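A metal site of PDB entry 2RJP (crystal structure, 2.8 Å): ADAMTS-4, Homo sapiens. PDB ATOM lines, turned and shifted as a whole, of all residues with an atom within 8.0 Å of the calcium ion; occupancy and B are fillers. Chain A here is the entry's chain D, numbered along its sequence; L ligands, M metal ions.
An oxygen (O4) of the ligand lies within hydrogen-bond range of the backbone NH of Leu 118, at 3.2 Å. The backbone NH (N) of Gly 119 sits at hydrogen-bond distance from an oxygen (O4) of the ligand, at 3.4 Å.
The side-chain hydroxyl (OG1) of Thr 117 is in hydrogen-bond range of the backbone NH (N) of Gly 111 (3.3 Å). The side-chain carboxylate of Glu 137 lies close to the backbone NH of Leu 109. The backbone NH of Glu 137 sits at hydrogen-bond distance from the backbone carbonyl oxygen of Leu 118 (2.8 Å). The backbone carbonyl oxygen (O) of Asp 108 lies within hydrogen-bond range of the side-chain sulfur (SG) of Cys 110, 3.4 Å away.
Within 4 Å of the calcium ion: Asp 108, Leu 109, Cys 115, Thr 117 and Glu 137.
O of Cys 115 is bound to the calcium ion. The calcium ion is bound by O of Thr 117 (2.4 Å). The calcium ion is bound by the side-chain carboxylate (OE1) of Glu 137 (2.5 Å). OD1 of Asp 108 is bound to the calcium ion. The calcium ion has four donor atoms within binding distance. Slightly farther from the calcium ion lies the backbone carbonyl oxygen (O) of Leu 109 (3.1 Å). Slightly farther from the calcium ion lies the side-chain carboxylate (OE2) of Glu 137 (3.1 Å).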
ATOM      1  N   PRO A  71     -15.810   0.227  14.992  1.00  0.00           N
ATOM      2  CA  PRO A  71     -14.365   0.207  14.702  1.00  0.00           C
ATOM      3  C   PRO A  71     -13.532   1.116  15.618  1.00  0.00           C
ATOM      4  O   PRO A  71     -12.434   0.731  16.019  1.00  0.00           O
ATOM      5  CB  PRO A  71     -14.292   0.692  13.242  1.00  0.00           C
ATOM      6  CG  PRO A  71     -15.586   1.383  12.998  1.00  0.00           C
ATOM      7  CD  PRO A  71     -16.595   0.656  13.822  1.00  0.00           C
ATOM      8  N   ARG A 106     -14.417  -9.614  18.574  1.00  0.00           N
ATOM      9  CA  ARG A 106     -13.674  -9.962  17.343  1.00  0.00           C
ATOM     10  C   ARG A 106     -13.566  -8.755  16.405  1.00  0.00           C
ATOM     11  O   ARG A 106     -12.817  -8.796  15.431  1.00  0.00           O
ATOM     12  CB  ARG A 106     -14.311 -11.149  16.585  1.00  0.00           C
ATOM     13  CG  ARG A 106     -14.247 -12.513  17.279  1.00  0.00           C
ATOM     14  CD  ARG A 106     -12.854 -12.896  17.789  1.00  0.00           C
ATOM     15  NE  ARG A 106     -11.927 -13.211  16.714  1.00  0.00           N
ATOM     16  CZ  ARG A 106     -10.931 -14.090  16.809  1.00  0.00           C
ATOM     17  NH1 ARG A 106     -10.737 -14.776  17.930  1.00  0.00           N
ATOM     18  NH2 ARG A 106     -10.136 -14.304  15.775  1.00  0.00           N
ATOM     19  N   GLN A 107     -14.330  -7.700  16.717  1.00  0.00           N
ATOM     20  CA  GLN A 107     -14.240  -6.435  16.009  1.00  0.00           C
ATOM     21  C   GLN A 107     -12.801  -5.960  15.966  1.00  0.00           C
ATOM     22  O   GLN A 107     -12.119  -5.944  16.991  1.00  0.00           O
ATOM     23  CB  GLN A 107     -15.115  -5.388  16.702  1.00  0.00           C
ATOM     24  CG  GLN A 107     -14.987  -3.962  16.160  1.00  0.00           C
ATOM     25  CD  GLN A 107     -15.537  -3.810  14.747  1.00  0.00           C
ATOM     26  OE1 GLN A 107     -16.725  -4.053  14.505  1.00  0.00           O
ATOM     27  NE2 GLN A 107     -14.684  -3.406  13.821  1.00  0.00           N
ATOM     28  N   ASP A 108     -12.328  -5.583  14.777  1.00  0.00           N
ATOM     29  CA  ASP A 108     -11.041  -4.933  14.654  1.00  0.00           C
ATOM     30  C   ASP A 108     -11.147  -3.521  15.222  1.00  0.00           C
ATOM     31  O   ASP A 108     -11.866  -2.664  14.679  1.00  0.00           O
ATOM     32  CB  ASP A 108     -10.560  -4.895  13.199  1.00  0.00           C
ATOM     33  CG  ASP A 108      -9.098  -4.487  13.063  1.00  0.00           C
ATOM     34  OD1 ASP A 108      -8.595  -3.718  13.915  1.00  0.00           O
ATOM     35  OD2 ASP A 108      -8.450  -4.945  12.101  1.00  0.00           O
ATOM     36  N   LEU A 109     -10.459  -3.290  16.330  1.00  0.00           N
ATOM     37  CA  LEU A 109     -10.457  -1.987  16.979  1.00  0.00           C
ATOM     38  C   LEU A 109      -9.411  -1.107  16.331  1.00  0.00           C
ATOM     39  O   LEU A 109      -8.334  -1.579  15.934  1.00  0.00           O
ATOM     40  CB  LEU A 109     -10.228  -2.133  18.482  1.00  0.00           C
ATOM     41  CG  LEU A 109     -11.246  -2.962  19.289  1.00  0.00           C
ATOM     42  CD1 LEU A 109     -10.712  -3.252  20.682  1.00  0.00           C
ATOM     43  CD2 LEU A 109     -12.604  -2.271  19.365  1.00  0.00           C
ATOM     44  N   CYS A 110      -9.732   0.187  16.229  1.00  0.00           N
ATOM     45  CA  CYS A 110      -8.909   1.137  15.474  1.00  0.00           C
ATOM     46  C   CYS A 110      -8.654   2.434  16.244  1.00  0.00           C
ATOM     47  O   CYS A 110      -9.455   2.832  17.099  1.00  0.00           O
ATOM     48  CB  CYS A 110      -9.575   1.454  14.134  1.00  0.00           C
ATOM     49  SG  CYS A 110     -10.248   0.013  13.245  1.00  0.00           S
ATOM     50  N   GLY A 111      -7.538   3.070  15.924  1.00  0.00           N
ATOM     51  CA  GLY A 111      -7.246   4.423  16.401  1.00  0.00           C
ATOM     52  C   GLY A 111      -7.592   5.403  15.306  1.00  0.00           C
ATOM     53  O   GLY A 111      -8.391   5.089  14.416  1.00  0.00           O
ATOM     54  N   THR A 114      -4.304   4.033  12.580  1.00  0.00           N
ATOM     55  CA  THR A 114      -4.179   2.608  12.265  1.00  0.00           C
ATOM     56  C   THR A 114      -5.200   1.727  12.993  1.00  0.00           C
ATOM     57  O   THR A 114      -5.863   2.162  13.937  1.00  0.00           O
ATOM     58  CB  THR A 114      -2.739   2.091  12.573  1.00  0.00           C
ATOM     59  OG1 THR A 114      -2.581   0.770  12.032  1.00  0.00           O
ATOM     60  CG2 THR A 114      -2.460   2.070  14.077  1.00  0.00           C
ATOM     61  N   CYS A 115      -5.300   0.473  12.543  1.00  0.00           N
ATOM     62  CA  CYS A 115      -6.134  -0.531  13.191  1.00  0.00           C
ATOM     63  C   CYS A 115      -5.282  -1.471  14.035  1.00  0.00           C
ATOM     64  O   CYS A 115      -5.779  -2.511  14.485  1.00  0.00           O
ATOM     65  CB  CYS A 115      -6.887  -1.335  12.157  1.00  0.00           C
ATOM     66  SG  CYS A 115      -7.991  -0.340  11.194  1.00  0.00           S
ATOM     67  N   ASP A 116      -4.025  -1.112  14.241  1.00  0.00           N
ATOM     68  CA  ASP A 116      -3.112  -1.946  15.014  1.00  0.00           C
ATOM     69  C   ASP A 116      -3.455  -1.952  16.517  1.00  0.00           C
ATOM     70  O   ASP A 116      -2.817  -2.657  17.305  1.00  0.00           O
ATOM     71  CB  ASP A 116      -1.648  -1.542  14.756  1.00  0.00           C
ATOM     72  CG  ASP A 116      -1.182  -1.859  13.342  1.00  0.00           C
ATOM     73  OD1 ASP A 116      -2.008  -2.257  12.495  1.00  0.00           O
ATOM     74  OD2 ASP A 116       0.024  -1.688  13.051  1.00  0.00           O
ATOM     75  N   THR A 117      -4.467  -1.164  16.886  1.00  0.00           N
ATOM     76  CA  THR A 117      -5.037  -1.178  18.237  1.00  0.00           C
ATOM     77  C   THR A 117      -5.500  -2.586  18.551  1.00  0.00           C
ATOM     78  O   THR A 117      -6.157  -3.224  17.721  1.00  0.00           O
ATOM     79  CB  THR A 117      -6.235  -0.221  18.359  1.00  0.00           C
ATOM     80  OG1 THR A 117      -5.873   1.072  17.873  1.00  0.00           O
ATOM     81  CG2 THR A 117      -6.687  -0.087  19.806  1.00  0.00           C
ATOM     82  N   LEU A 118      -5.132  -3.073  19.736  1.00  0.00           N
ATOM     83  CA  LEU A 118      -5.531  -4.401  20.204  1.00  0.00           C
ATOM     84  C   LEU A 118      -6.446  -4.345  21.424  1.00  0.00           C
ATOM     85  O   LEU A 118      -7.081  -5.333  21.786  1.00  0.00           O
ATOM     86  CB  LEU A 118      -4.300  -5.271  20.498  1.00  0.00           C
ATOM     87  CG  LEU A 118      -3.606  -5.962  19.327  1.00  0.00           C
ATOM     88  CD1 LEU A 118      -2.614  -6.987  19.840  1.00  0.00           C
ATOM     89  CD2 LEU A 118      -4.602  -6.617  18.377  1.00  0.00           C
ATOM     90  N   GLY A 119      -6.495  -3.176  22.066  1.00  0.00           N
ATOM     91  CA  GLY A 119      -7.355  -2.937  23.214  1.00  0.00           C
ATOM     92  C   GLY A 119      -7.268  -1.495  23.671  1.00  0.00           C
ATOM     93  O   GLY A 119      -6.413  -0.732  23.209  1.00  0.00           O
ATOM     94  N   GLU A 137      -9.550  -6.598  21.857  1.00  0.00           N
ATOM     95  CA  GLU A 137      -9.774  -7.294  20.598  1.00  0.00           C
ATOM     96  C   GLU A 137      -9.170  -8.682  20.705  1.00  0.00           C
ATOM     97  O   GLU A 137      -7.988  -8.826  21.043  1.00  0.00           O
ATOM     98  CB  GLU A 137      -9.112  -6.536  19.438  1.00  0.00           C
ATOM     99  CG  GLU A 137      -9.048  -7.319  18.143  1.00  0.00           C
ATOM    100  CD  GLU A 137      -8.441  -6.522  17.017  1.00  0.00           C
ATOM    101  OE1 GLU A 137      -8.567  -5.281  17.018  1.00  0.00           O
ATOM    102  OE2 GLU A 137      -7.813  -7.136  16.120  1.00  0.00           O
ATOM    103  N   ASP A 138      -9.975  -9.691  20.436  1.00  0.00           N
ATOM    104  CA  ASP A 138      -9.521 -11.062  20.498  1.00  0.00           C
ATOM    105  C   ASP A 138      -8.911 -11.442  19.155  1.00  0.00           C
ATOM    106  O   ASP A 138      -9.629 -11.644  18.171  1.00  0.00           O
ATOM    107  CB  ASP A 138     -10.694 -11.978  20.848  1.00  0.00           C
ATOM    108  CG  ASP A 138     -10.364 -13.457  20.701  1.00  0.00           C
ATOM    109  OD1 ASP A 138      -9.181 -13.839  20.791  1.00  0.00           O
ATOM    110  OD2 ASP A 138     -11.299 -14.244  20.498  1.00  0.00           O
ATOM    111  N   ASP A 139      -7.582 -11.527  19.125  1.00  0.00           N
ATOM    112  CA  ASP A 139      -6.838 -11.977  17.957  1.00  0.00           C
ATOM    113  C   ASP A 139      -6.225 -13.360  18.249  1.00  0.00           C
ATOM    114  O   ASP A 139      -5.145 -13.707  17.761  1.00  0.00           O
ATOM    115  CB  ASP A 139      -5.743 -10.956  17.577  1.00  0.00           C
ATOM    116  CG  ASP A 139      -4.688 -10.768  18.672  1.00  0.00           C
ATOM    117  OD1 ASP A 139      -4.936 -11.162  19.838  1.00  0.00           O
ATOM    118  OD2 ASP A 139      -3.601 -10.231  18.365  1.00  0.00           O
ATOM    119  N   LYS A 273       1.606 -13.762  13.436  1.00  0.00           N
ATOM    120  CA  LYS A 273       1.495 -12.564  14.267  1.00  0.00           C
ATOM    121  C   LYS A 273       2.638 -12.540  15.290  1.00  0.00           C
ATOM    122  O   LYS A 273       2.650 -11.706  16.214  1.00  0.00           O
ATOM    123  CB  LYS A 273       0.125 -12.489  14.946  1.00  0.00           C
ATOM    124  CG  LYS A 273      -0.972 -11.888  14.073  1.00  0.00           C
ATOM    125  CD  LYS A 273      -2.105 -11.344  14.924  1.00  0.00           C
ATOM    126  CE  LYS A 273      -2.689 -10.071  14.322  1.00  0.00           C
ATOM    127  NZ  LYS A 273      -3.273  -9.187  15.391  1.00  0.00           N
HETATM  128  C1  LIG L   1      -5.298   2.865  23.035  1.00  0.00           C
HETATM  129  C2  LIG L   1      -3.830   2.679  23.456  1.00  0.00           C
HETATM  130  C3  LIG L   1      -3.516   3.605  24.633  1.00  0.00           C
HETATM  131  C4  LIG L   1      -3.520   1.173  23.661  1.00  0.00           C
HETATM  132  C5  LIG L   1      -3.097   0.758  25.120  1.00  0.00           C
HETATM  133  O1  LIG L   1      -1.847   0.865  25.350  1.00  0.00           O
HETATM  134  O2  LIG L   1      -4.022   0.360  25.882  1.00  0.00           O
HETATM  135  N1  LIG L   1      -2.353   0.809  22.745  1.00  0.00           N
HETATM  136  S1  LIG L   1      -2.518  -0.575  21.792  1.00  0.00           S
HETATM  137  O3  LIG L   1      -1.763  -0.330  20.576  1.00  0.00           O
HETATM  138  O4  LIG L   1      -3.934  -0.901  21.682  1.00  0.00           O
HETATM  139  C6  LIG L   1      -1.711  -1.899  22.635  1.00  0.00           C
HETATM  140  C7  LIG L   1      -0.364  -1.780  22.990  1.00  0.00           C
HETATM  141  C8  LIG L   1       0.281  -2.836  23.638  1.00  0.00           C
HETATM  142  C9  LIG L   1      -0.400  -4.033  23.959  1.00  0.00           C
HETATM  143  C10 LIG L   1      -1.756  -4.129  23.578  1.00  0.00           C
HETATM  144  C11 LIG L   1      -2.407  -3.077  22.918  1.00  0.00           C
HETATM  145  C12 LIG L   1       0.287  -5.155  24.625  1.00  0.00           C
HETATM  146  C13 LIG L   1      -0.346  -6.413  24.748  1.00  0.00           C
HETATM  147  C14 LIG L   1       0.296  -7.499  25.354  1.00  0.00           C
HETATM  148  C15 LIG L   1       1.607  -7.365  25.850  1.00  0.00           C
HETATM  149  C16 LIG L   1       2.247  -6.127  25.719  1.00  0.00           C
HETATM  150  C17 LIG L   1       1.598  -5.046  25.119  1.00  0.00           C
HETATM  151  C18 LIG L   1       2.301  -8.532  26.507  1.00  0.00           C
HETATM  152  O5  LIG L   1       1.748  -8.711  27.805  1.00  0.00           O
HETATM  153  C19 LIG L   1       1.821  -9.891  28.511  1.00  0.00           C
HETATM  154  C20 LIG L   1       0.997 -10.164  29.606  1.00  0.00           C
HETATM  155  C21 LIG L   1       1.119 -11.390  30.301  1.00  0.00           C
HETATM  156  C22 LIG L   1       2.064 -12.351  29.912  1.00  0.00           C
HETATM  157  C23 LIG L   1       2.881 -12.082  28.805  1.00  0.00           C
HETATM  158  C24 LIG L   1       2.767 -10.853  28.121  1.00  0.00           C
HETATM  159  C25 LIG L   1       2.180 -13.657  30.642  1.00  0.00           C
HETATM  160  O6  LIG L   1       1.129 -14.224  30.969  1.00  0.00           O
HETATM  161  C26 LIG L   1       3.537 -14.158  31.157  1.00  0.00           C
HETATM  162  C27 LIG L   1       4.029 -15.326  30.299  1.00  0.00           C
HETATM  163  C28 LIG L   1       3.408 -14.594  32.623  1.00  0.00           C
HETATM  164 CA    CA M   1      -6.809  -4.242  15.643  1.00  0.00          CA
